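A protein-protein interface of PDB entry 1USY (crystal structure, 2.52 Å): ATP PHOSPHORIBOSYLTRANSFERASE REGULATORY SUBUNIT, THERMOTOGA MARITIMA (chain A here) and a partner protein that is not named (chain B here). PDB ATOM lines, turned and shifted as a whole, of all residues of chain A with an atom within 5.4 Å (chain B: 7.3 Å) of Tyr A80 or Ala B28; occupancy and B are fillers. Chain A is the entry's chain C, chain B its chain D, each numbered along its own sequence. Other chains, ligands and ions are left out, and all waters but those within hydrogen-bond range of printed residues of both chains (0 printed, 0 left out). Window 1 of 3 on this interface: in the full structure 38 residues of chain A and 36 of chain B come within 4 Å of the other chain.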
ATOM      1  N   ALA A  28       1.270   5.711  -9.553  1.00  0.00           N
ATOM      2  CA  ALA A  28       1.711   5.129 -10.821  1.00  0.00           C
ATOM      3  C   ALA A  28       0.599   5.102 -11.869  1.00  0.00           C
ATOM      4  O   ALA A  28       0.847   5.215 -13.063  1.00  0.00           O
ATOM      5  CB  ALA A  28       2.232   3.747 -10.598  1.00  0.00           C
ATOM      6  N   LEU A  29      -0.635   4.947 -11.424  1.00  0.00           N
ATOM      7  CA  LEU A  29      -1.696   4.823 -12.388  1.00  0.00           C
ATOM      8  C   LEU A  29      -2.277   6.184 -12.699  1.00  0.00           C
ATOM      9  O   LEU A  29      -2.268   7.086 -11.847  1.00  0.00           O
ATOM     10  CB  LEU A  29      -2.741   3.863 -11.880  1.00  0.00           C
ATOM     11  CG  LEU A  29      -2.353   2.461 -12.299  1.00  0.00           C
ATOM     12  CD1 LEU A  29      -2.735   1.518 -11.211  1.00  0.00           C
ATOM     13  CD2 LEU A  29      -3.040   2.082 -13.596  1.00  0.00           C
ATOM     14  N   ILE A  50      -0.250   3.373 -17.198  1.00  0.00           N
ATOM     15  CA  ILE A  50       0.682   3.160 -16.094  1.00  0.00           C
ATOM     16  C   ILE A  50       2.016   3.839 -16.332  1.00  0.00           C
ATOM     17  O   ILE A  50       2.513   3.866 -17.446  1.00  0.00           O
ATOM     18  CB  ILE A  50       0.856   1.651 -15.804  1.00  0.00           C
ATOM     19  CG1 ILE A  50       1.642   1.466 -14.520  1.00  0.00           C
ATOM     20  CG2 ILE A  50       1.568   0.941 -16.931  1.00  0.00           C
ATOM     21  CD1 ILE A  50       1.258   0.247 -13.726  1.00  0.00           C
ATOM     22  N   ARG A  51       2.602   4.386 -15.281  1.00  0.00           N
ATOM     23  CA  ARG A  51       3.862   5.102 -15.401  1.00  0.00           C
ATOM     24  C   ARG A  51       4.970   4.279 -16.108  1.00  0.00           C
ATOM     25  O   ARG A  51       5.408   3.215 -15.626  1.00  0.00           O
ATOM     26  CB  ARG A  51       4.316   5.581 -14.034  1.00  0.00           C
ATOM     27  CG  ARG A  51       5.674   6.251 -14.048  1.00  0.00           C
ATOM     28  CD  ARG A  51       6.316   6.274 -12.683  1.00  0.00           C
ATOM     29  NE  ARG A  51       5.415   6.892 -11.719  1.00  0.00           N
ATOM     30  CZ  ARG A  51       5.166   6.397 -10.523  1.00  0.00           C
ATOM     31  NH1 ARG A  51       5.747   5.270 -10.121  1.00  0.00           N
ATOM     32  NH2 ARG A  51       4.333   7.038  -9.720  1.00  0.00           N
ATOM     33  N   GLU A  52       5.393   4.768 -17.270  1.00  0.00           N
ATOM     34  CA  GLU A  52       6.339   4.042 -18.089  1.00  0.00           C
ATOM     35  C   GLU A  52       7.618   4.832 -18.315  1.00  0.00           C
ATOM     36  O   GLU A  52       8.647   4.279 -18.740  1.00  0.00           O
ATOM     37  CB  GLU A  52       5.669   3.651 -19.398  1.00  0.00           C
ATOM     38  CG  GLU A  52       4.866   2.370 -19.241  1.00  0.00           C
ATOM     39  CD  GLU A  52       4.069   1.991 -20.466  1.00  0.00           C
ATOM     40  OE1 GLU A  52       2.877   2.379 -20.552  1.00  0.00           O
ATOM     41  OE2 GLU A  52       4.636   1.284 -21.336  1.00  0.00           O
ATOM     42  N   ASP A  77      10.863   5.412  -7.394  1.00  0.00           N
ATOM     43  CA  ASP A  77       9.623   4.692  -7.584  1.00  0.00           C
ATOM     44  C   ASP A  77       9.695   3.687  -8.695  1.00  0.00           C
ATOM     45  O   ASP A  77      10.610   3.711  -9.492  1.00  0.00           O
ATOM     46  CB  ASP A  77       8.489   5.667  -7.898  1.00  0.00           C
ATOM     47  CG  ASP A  77       7.156   5.178  -7.388  1.00  0.00           C
ATOM     48  OD1 ASP A  77       6.407   6.031  -6.895  1.00  0.00           O
ATOM     49  OD2 ASP A  77       6.775   3.972  -7.414  1.00  0.00           O
ATOM     50  N   PHE A  78       8.675   2.847  -8.766  1.00  0.00           N
ATOM     51  CA  PHE A  78       8.581   1.853  -9.806  1.00  0.00           C
ATOM     52  C   PHE A  78       8.245   2.497 -11.140  1.00  0.00           C
ATOM     53  O   PHE A  78       7.352   3.305 -11.234  1.00  0.00           O
ATOM     54  CB  PHE A  78       7.585   0.727  -9.392  1.00  0.00           C
ATOM     55  CG  PHE A  78       8.114  -0.146  -8.281  1.00  0.00           C
ATOM     56  CD1 PHE A  78       7.635  -0.025  -7.003  1.00  0.00           C
ATOM     57  CD2 PHE A  78       9.176  -1.030  -8.507  1.00  0.00           C
ATOM     58  CE1 PHE A  78       8.151  -0.800  -5.965  1.00  0.00           C
ATOM     59  CE2 PHE A  78       9.708  -1.814  -7.476  1.00  0.00           C
ATOM     60  CZ  PHE A  78       9.198  -1.716  -6.212  1.00  0.00           C
ATOM     61  N   VAL A  79       8.990   2.146 -12.171  1.00  0.00           N
ATOM     62  CA  VAL A  79       8.584   2.426 -13.540  1.00  0.00           C
ATOM     63  C   VAL A  79       8.217   1.050 -14.143  1.00  0.00           C
ATOM     64  O   VAL A  79       8.903   0.052 -13.858  1.00  0.00           O
ATOM     65  CB  VAL A  79       9.714   3.090 -14.292  1.00  0.00           C
ATOM     66  CG1 VAL A  79       9.446   3.066 -15.761  1.00  0.00           C
ATOM     67  CG2 VAL A  79       9.954   4.544 -13.764  1.00  0.00           C
ATOM     68  N   TYR A  80       7.106   0.982 -14.891  1.00  0.00           N
ATOM     69  CA  TYR A  80       6.558  -0.290 -15.398  1.00  0.00           C
ATOM     70  C   TYR A  80       6.793  -0.362 -16.916  1.00  0.00           C
ATOM     71  O   TYR A  80       6.916   0.679 -17.597  1.00  0.00           O
ATOM     72  CB  TYR A  80       5.045  -0.469 -15.046  1.00  0.00           C
ATOM     73  CG  TYR A  80       4.698  -0.267 -13.563  1.00  0.00           C
ATOM     74  CD1 TYR A  80       4.930   0.957 -12.924  1.00  0.00           C
ATOM     75  CD2 TYR A  80       4.161  -1.294 -12.801  1.00  0.00           C
ATOM     76  CE1 TYR A  80       4.652   1.136 -11.571  1.00  0.00           C
ATOM     77  CE2 TYR A  80       3.848  -1.111 -11.441  1.00  0.00           C
ATOM     78  CZ  TYR A  80       4.113   0.095 -10.823  1.00  0.00           C
ATOM     79  OH  TYR A  80       3.824   0.288  -9.467  1.00  0.00           O
ATOM     80  N   ARG A  81       6.892  -1.594 -17.424  1.00  0.00           N
ATOM     81  CA  ARG A  81       7.128  -1.863 -18.831  1.00  0.00           C
ATOM     82  C   ARG A  81       6.687  -3.286 -19.051  1.00  0.00           C
ATOM     83  O   ARG A  81       6.479  -4.015 -18.078  1.00  0.00           O
ATOM     84  CB  ARG A  81       8.612  -1.662 -19.226  1.00  0.00           C
ATOM     85  CG  ARG A  81       9.434  -2.951 -19.380  1.00  0.00           C
ATOM     86  CD  ARG A  81      10.954  -2.753 -19.499  1.00  0.00           C
ATOM     87  NE  ARG A  81      11.723  -3.902 -18.979  1.00  0.00           N
ATOM     88  CZ  ARG A  81      12.233  -3.985 -17.737  1.00  0.00           C
ATOM     89  NH1 ARG A  81      12.046  -3.018 -16.847  1.00  0.00           N
ATOM     90  NH2 ARG A  81      12.922  -5.049 -17.369  1.00  0.00           N
ATOM     91  N   TYR A  82       6.524  -3.671 -20.323  1.00  0.00           N
ATOM     92  CA  TYR A  82       6.165  -5.039 -20.683  1.00  0.00           C
ATOM     93  C   TYR A  82       7.383  -5.844 -21.174  1.00  0.00           C
ATOM     94  O   TYR A  82       8.105  -5.402 -22.059  1.00  0.00           O
ATOM     95  CB  TYR A  82       5.053  -5.035 -21.740  1.00  0.00           C
ATOM     96  CG  TYR A  82       3.670  -4.870 -21.143  1.00  0.00           C
ATOM     97  CD1 TYR A  82       3.051  -3.635 -21.117  1.00  0.00           C
ATOM     98  CD2 TYR A  82       2.995  -5.953 -20.579  1.00  0.00           C
ATOM     99  CE1 TYR A  82       1.788  -3.487 -20.540  1.00  0.00           C
ATOM    100  CE2 TYR A  82       1.772  -5.816 -19.997  1.00  0.00           C
ATOM    101  CZ  TYR A  82       1.163  -4.583 -19.978  1.00  0.00           C
ATOM    102  OH  TYR A  82      -0.095  -4.453 -19.428  1.00  0.00           O
ATOM    103  N   LEU A  87       3.948  -7.976 -17.101  1.00  0.00           N
ATOM    104  CA  LEU A  87       4.186  -6.632 -16.586  1.00  0.00           C
ATOM    105  C   LEU A  87       5.356  -6.615 -15.625  1.00  0.00           C
ATOM    106  O   LEU A  87       5.337  -7.320 -14.634  1.00  0.00           O
ATOM    107  CB  LEU A  87       2.950  -6.121 -15.860  1.00  0.00           C
ATOM    108  CG  LEU A  87       2.451  -4.695 -16.049  1.00  0.00           C
ATOM    109  CD1 LEU A  87       1.955  -4.209 -14.709  1.00  0.00           C
ATOM    110  CD2 LEU A  87       3.524  -3.770 -16.621  1.00  0.00           C
ATOM    111  N   VAL A  88       6.382  -5.824 -15.890  1.00  0.00           N
ATOM    112  CA  VAL A  88       7.485  -5.786 -14.937  1.00  0.00           C
ATOM    113  C   VAL A  88       7.777  -4.374 -14.520  1.00  0.00           C
ATOM    114  O   VAL A  88       7.378  -3.431 -15.195  1.00  0.00           O
ATOM    115  CB  VAL A  88       8.788  -6.502 -15.441  1.00  0.00           C
ATOM    116  CG1 VAL A  88       8.460  -7.856 -16.086  1.00  0.00           C
ATOM    117  CG2 VAL A  88       9.588  -5.634 -16.369  1.00  0.00           C
ATOM    118  N   ALA A  89       8.498  -4.221 -13.420  1.00  0.00           N
ATOM    119  CA  ALA A  89       8.635  -2.928 -12.839  1.00  0.00           C
ATOM    120  C   ALA A  89      10.078  -2.731 -12.440  1.00  0.00           C
ATOM    121  O   ALA A  89      10.692  -3.628 -11.876  1.00  0.00           O
ATOM    122  CB  ALA A  89       7.659  -2.786 -11.631  1.00  0.00           C
ATOM    123  N   GLU A  90      10.610  -1.548 -12.752  1.00  0.00           N
ATOM    124  CA  GLU A  90      11.949  -1.168 -12.335  1.00  0.00           C
ATOM    125  C   GLU A  90      11.837  -0.093 -11.299  1.00  0.00           C
ATOM    126  O   GLU A  90      11.240   0.935 -11.560  1.00  0.00           O
ATOM    127  CB  GLU A  90      12.747  -0.598 -13.512  1.00  0.00           C
ATOM    128  CG  GLU A  90      13.968  -1.409 -13.904  1.00  0.00           C
ATOM    129  CD  GLU A  90      15.054  -1.397 -12.849  1.00  0.00           C
ATOM    130  OE1 GLU A  90      15.799  -2.396 -12.735  1.00  0.00           O
ATOM    131  OE2 GLU A  90      15.168  -0.385 -12.123  1.00  0.00           O
ATOM    132  N   VAL B  26       6.802  -2.961  -2.955  1.00  0.00           N
ATOM    133  CA  VAL B  26       6.267  -3.738  -4.064  1.00  0.00           C
ATOM    134  C   VAL B  26       5.600  -2.846  -5.100  1.00  0.00           C
ATOM    135  O   VAL B  26       5.116  -1.780  -4.739  1.00  0.00           O
ATOM    136  CB  VAL B  26       5.230  -4.792  -3.566  1.00  0.00           C
ATOM    137  CG1 VAL B  26       5.955  -5.982  -2.853  1.00  0.00           C
ATOM    138  CG2 VAL B  26       4.195  -4.160  -2.680  1.00  0.00           C
ATOM    139  N   PRO B  27       5.526  -3.288  -6.360  1.00  0.00           N
ATOM    140  CA  PRO B  27       4.740  -2.582  -7.391  1.00  0.00           C
ATOM    141  C   PRO B  27       3.277  -2.357  -6.981  1.00  0.00           C
ATOM    142  O   PRO B  27       2.755  -3.106  -6.178  1.00  0.00           O
ATOM    143  CB  PRO B  27       4.767  -3.534  -8.577  1.00  0.00           C
ATOM    144  CG  PRO B  27       5.938  -4.359  -8.384  1.00  0.00           C
ATOM    145  CD  PRO B  27       6.177  -4.494  -6.904  1.00  0.00           C
ATOM    146  N   ALA B  28       2.642  -1.324  -7.523  1.00  0.00           N
ATOM    147  CA  ALA B  28       1.249  -1.038  -7.222  1.00  0.00           C
ATOM    148  C   ALA B  28       0.350  -2.160  -7.802  1.00  0.00           C
ATOM    149  O   ALA B  28      -0.567  -2.623  -7.146  1.00  0.00           O
ATOM    150  CB  ALA B  28       0.861   0.347  -7.783  1.00  0.00           C
ATOM    151  N   LEU B  29       0.615  -2.597  -9.029  1.00  0.00           N
ATOM    152  CA  LEU B  29      -0.103  -3.742  -9.564  1.00  0.00           C
ATOM    153  C   LEU B  29       0.545  -5.070  -9.202  1.00  0.00           C
ATOM    154  O   LEU B  29       1.769  -5.195  -9.125  1.00  0.00           O
ATOM    155  CB  LEU B  29      -0.298  -3.634 -11.075  1.00  0.00           C
ATOM    156  CG  LEU B  29      -1.110  -2.399 -11.441  1.00  0.00           C
ATOM    157  CD1 LEU B  29      -1.274  -2.284 -12.946  1.00  0.00           C
ATOM    158  CD2 LEU B  29      -2.461  -2.429 -10.748  1.00  0.00           C
ATOM    159  N   GLU B  30      -0.244  -6.024  -9.021  1.00  0.00           N
ATOM    160  CA  GLU B  30       0.063  -7.402  -8.633  1.00  0.00           C
ATOM    161  C   GLU B  30      -0.838  -8.356  -9.375  1.00  0.00           C
ATOM    162  O   GLU B  30      -2.060  -8.274  -9.251  1.00  0.00           O
ATOM    163  CB  GLU B  30      -0.194  -7.567  -7.159  1.00  0.00           C
ATOM    164  CG  GLU B  30       0.693  -8.574  -6.472  1.00  0.00           C
ATOM    165  CD  GLU B  30       0.648  -8.360  -4.982  1.00  0.00           C
ATOM    166  OE1 GLU B  30       1.367  -7.434  -4.463  1.00  0.00           O
ATOM    167  OE2 GLU B  30      -0.118  -9.096  -4.255  1.00  0.00           O
ATOM    168  N   LYS B  31      -0.210  -9.236 -10.125  1.00  0.00           N
ATOM    169  CA  LYS B  31      -0.922 -10.258 -10.913  1.00  0.00           C
ATOM    170  C   LYS B  31      -1.785 -11.126  -9.977  1.00  0.00           C
ATOM    171  O   LYS B  31      -1.379 -11.488  -8.869  1.00  0.00           O
ATOM    172  CB  LYS B  31       0.087 -11.142 -11.629  1.00  0.00           C
ATOM    173  CG  LYS B  31      -0.444 -11.698 -12.938  1.00  0.00           C
ATOM    174  CD  LYS B  31       0.618 -12.445 -13.734  1.00  0.00           C
ATOM    175  CE  LYS B  31       0.021 -13.467 -14.696  1.00  0.00           C
ATOM    176  NZ  LYS B  31       0.647 -14.792 -14.583  1.00  0.00           N
ATOM    177  N   PHE B  48      -4.980  -7.864 -12.989  1.00  0.00           N
ATOM    178  CA  PHE B  48      -4.282  -7.406 -11.817  1.00  0.00           C
ATOM    179  C   PHE B  48      -5.228  -6.876 -10.753  1.00  0.00           C
ATOM    180  O   PHE B  48      -6.316  -6.394 -11.063  1.00  0.00           O
ATOM    181  CB  PHE B  48      -3.293  -6.286 -12.141  1.00  0.00           C
ATOM    182  CG  PHE B  48      -2.418  -6.537 -13.331  1.00  0.00           C
ATOM    183  CD1 PHE B  48      -2.810  -6.099 -14.593  1.00  0.00           C
ATOM    184  CD2 PHE B  48      -1.184  -7.143 -13.187  1.00  0.00           C
ATOM    185  CE1 PHE B  48      -2.000  -6.308 -15.713  1.00  0.00           C
ATOM    186  CE2 PHE B  48      -0.356  -7.345 -14.289  1.00  0.00           C
ATOM    187  CZ  PHE B  48      -0.776  -6.917 -15.563  1.00  0.00           C
ATOM    188  N   SER B  49      -4.786  -6.962  -9.502  1.00  0.00           N
ATOM    189  CA  SER B  49      -5.366  -6.220  -8.402  1.00  0.00           C
ATOM    190  C   SER B  49      -4.414  -5.096  -8.067  1.00  0.00           C
ATOM    191  O   SER B  49      -3.198  -5.237  -8.242  1.00  0.00           O
ATOM    192  CB  SER B  49      -5.519  -7.120  -7.168  1.00  0.00           C
ATOM    193  OG  SER B  49      -4.275  -7.704  -6.801  1.00  0.00           O
ATOM    194  N   ILE B  50      -4.973  -3.994  -7.567  1.00  0.00           N
ATOM    195  CA  ILE B  50      -4.215  -2.831  -7.090  1.00  0.00           C
ATOM    196  C   ILE B  50      -4.131  -2.807  -5.567  1.00  0.00           C
ATOM    197  O   ILE B  50      -5.036  -3.287  -4.870  1.00  0.00           O
ATOM    198  CB  ILE B  50      -4.842  -1.498  -7.607  1.00  0.00           C
ATOM    199  CG1 ILE B  50      -3.767  -0.403  -7.664  1.00  0.00           C
ATOM    200  CG2 ILE B  50      -6.010  -1.046  -6.713  1.00  0.00           C
ATOM    201  CD1 ILE B  50      -4.139   0.783  -8.526  1.00  0.00           C
ATOM    202  N   ARG B  51      -3.053  -2.219  -5.064  1.00  0.00           N
ATOM    203  CA  ARG B  51      -2.826  -2.101  -3.631  1.00  0.00           C
ATOM    204  C   ARG B  51      -3.939  -1.307  -2.950  1.00  0.00           C
ATOM    205  O   ARG B  51      -4.049  -0.096  -3.107  1.00  0.00           O
ATOM    206  CB  ARG B  51      -1.471  -1.455  -3.371  1.00  0.00           C
ATOM    207  CG  ARG B  51      -0.991  -1.662  -1.980  1.00  0.00           C
ATOM    208  CD  ARG B  51       0.152  -0.811  -1.687  1.00  0.00           C
ATOM    209  NE  ARG B  51       1.244  -1.177  -2.578  1.00  0.00           N
ATOM    210  CZ  ARG B  51       1.957  -0.323  -3.305  1.00  0.00           C
ATOM    211  NH1 ARG B  51       1.715   0.979  -3.249  1.00  0.00           N
ATOM    212  NH2 ARG B  51       2.925  -0.786  -4.079  1.00  0.00           N
ATOM    213  N   GLU B  52      -4.779  -2.011  -2.208  1.00  0.00           N
ATOM    214  CA  GLU B  52      -5.949  -1.403  -1.593  1.00  0.00           C
ATOM    215  C   GLU B  52      -5.813  -1.416  -0.099  1.00  0.00           C
ATOM    216  O   GLU B  52      -6.524  -0.705   0.607  1.00  0.00           O
ATOM    217  CB  GLU B  52      -7.202  -2.170  -1.988  1.00  0.00           C
ATOM    218  CG  GLU B  52      -7.735  -1.735  -3.316  1.00  0.00           C
ATOM    219  CD  GLU B  52      -8.831  -2.630  -3.855  1.00  0.00           C
ATOM    220  OE1 GLU B  52      -9.948  -2.135  -4.040  1.00  0.00           O
ATOM    221  OE2 GLU B  52      -8.568  -3.812  -4.144  1.00  0.00           O
ATOM    222  N   THR B  57      -1.667  -7.035   1.427  1.00  0.00           N
ATOM    223  CA  THR B  57      -0.512  -7.161   0.559  1.00  0.00           C
ATOM    224  C   THR B  57       0.687  -7.816   1.275  1.00  0.00           C
ATOM    225  O   THR B  57       1.259  -8.790   0.744  1.00  0.00           O
ATOM    226  CB  THR B  57      -0.195  -5.761  -0.018  1.00  0.00           C
ATOM    227  OG1 THR B  57      -1.290  -5.362  -0.859  1.00  0.00           O
ATOM    228  CG2 THR B  57       0.997  -5.782  -0.983  1.00  0.00           C
ATOM    229  N   ASP B  77       4.268   4.111   0.497  1.00  0.00           N
ATOM    230  CA  ASP B  77       3.789   4.154  -0.879  1.00  0.00           C
ATOM    231  C   ASP B  77       2.300   4.520  -1.011  1.00  0.00           C
ATOM    232  O   ASP B  77       1.571   4.667  -0.026  1.00  0.00           O
ATOM    233  CB  ASP B  77       4.040   2.817  -1.626  1.00  0.00           C
ATOM    234  CG  ASP B  77       4.260   3.025  -3.116  1.00  0.00           C
ATOM    235  OD1 ASP B  77       4.676   4.141  -3.526  1.00  0.00           O
ATOM    236  OD2 ASP B  77       4.058   2.154  -3.967  1.00  0.00           O
ATOM    237  N   PHE B  78       1.851   4.627  -2.249  1.00  0.00           N
ATOM    238  CA  PHE B  78       0.465   4.888  -2.512  1.00  0.00           C
ATOM    239  C   PHE B  78      -0.416   3.696  -2.283  1.00  0.00           C
ATOM    240  O   PHE B  78      -0.021   2.577  -2.574  1.00  0.00           O
ATOM    241  CB  PHE B  78       0.299   5.396  -3.940  1.00  0.00           C
ATOM    242  CG  PHE B  78       0.812   6.736  -4.098  1.00  0.00           C
ATOM    243  CD1 PHE B  78       2.107   6.925  -4.528  1.00  0.00           C
ATOM    244  CD2 PHE B  78       0.042   7.830  -3.689  1.00  0.00           C
ATOM    245  CE1 PHE B  78       2.621   8.217  -4.647  1.00  0.00           C
ATOM    246  CE2 PHE B  78       0.538   9.126  -3.794  1.00  0.00           C
ATOM    247  CZ  PHE B  78       1.834   9.325  -4.286  1.00  0.00           C
ATOM    248  N   TYR B  80      -4.361   2.714  -3.227  1.00  0.00           N
ATOM    249  CA  TYR B  80      -5.420   3.147  -4.144  1.00  0.00           C
ATOM    250  C   TYR B  80      -6.789   2.762  -3.603  1.00  0.00           C
ATOM    251  O   TYR B  80      -6.926   1.772  -2.889  1.00  0.00           O
ATOM    252  CB  TYR B  80      -5.186   2.572  -5.545  1.00  0.00           C
ATOM    253  CG  TYR B  80      -3.848   2.991  -6.115  1.00  0.00           C
ATOM    254  CD1 TYR B  80      -2.668   2.454  -5.615  1.00  0.00           C
ATOM    255  CD2 TYR B  80      -3.762   3.949  -7.120  1.00  0.00           C
ATOM    256  CE1 TYR B  80      -1.482   2.813  -6.099  1.00  0.00           C
ATOM    257  CE2 TYR B  80      -2.536   4.338  -7.613  1.00  0.00           C
ATOM    258  CZ  TYR B  80      -1.400   3.750  -7.091  1.00  0.00           C
ATOM    259  OH  TYR B  80      -0.138   4.085  -7.522  1.00  0.00           O
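N of Ala B28 lies within hydrogen-bond range of OH of Tyr A80. The side-chain hydroxyl (OH) of Tyr B80 is in hydrogen-bond range of the backbone NH (N) of Ala A28 (3.0 Å).
Leu B29 touches Leu A29 (CD2 to CD1, 3.98 Å). CD1 of Ile B50 touches CD1 of Leu A29, at 3.1 Å. Leu B29 touches Ile A50 (CD1 to CD1, 3.7 Å). Phe A78 touches Val B26 (CE1 to C, 3.4 Å). Pro B27 touches Phe A78. CA of Pro B27 touches OH of Tyr A80, 3.7 Å away. CZ of Phe B48 touches CB of Leu A87, at 3.8 Å. CG of Pro B27 touches CB of Ala A89, 3.997 Å away.
Of chain B, only Pro B27 and Ala B28 come within 4 Å of Tyr A80. Of chain A, only Tyr A80 (2.8 Å) comes within 4 Å of Ala B28. Of the printed residues of chain A, Pro B27 touches Phe A78, Tyr A80 and Ala A89. Printed residues of chain B within 4 Å of Phe A78: Val B26 and Pro B27. Printed residues of chain A within 4 Å of Ile B50: Leu A29. Printed residues of chain A within 4 Å of Phe B48: Leu A87. Glu B30 touches none of the printed residues of chain A. The nearest printed residue of chain A that does not touch Val B26 is Tyr A80 (5.3 Å).
The backbone carbonyl oxygen of Val B26 lies within hydrogen-bond range of the guanidinium group of Arg B51. The backbone NH (N) of Tyr A80 sits at hydrogen-bond distance from the backbone carbonyl oxygen (O) of Arg A51 (2.9 Å). NH1 of Arg A51 is in hydrogen-bond range of O of Phe A78 (2.8 Å). O of Ala A28 is in hydrogen-bond range of N of Arg A51 (2.9 Å). The backbone NH (N) of Arg B51 is in hydrogen-bond range of the backbone carbonyl oxygen (O) of Ala B28. The backbone carbonyl oxygen of Pro B27 is in hydrogen-bond range of the guanidinium group of Arg B51, at 3.1 Å.
Along chain A the printed residues that touch a printed residue of chain B span positions 28 to 89. Of the 15 printed residues of chain B, 7 touch a printed residue of chain A. Printed residues of chain B that touch a printed residue of chain A: Val B26, Pro B27, Ala B28, Leu B29, Phe B48, Ile B50 and Tyr B80. Hydrophobic or aromatic side chains of chain B that line the printed part of chain A: Pro B27, Ala B28, Leu B29, Phe B48, Ile B50 and Tyr B80. Among the printed residues, 10 pairs touch across the chains.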
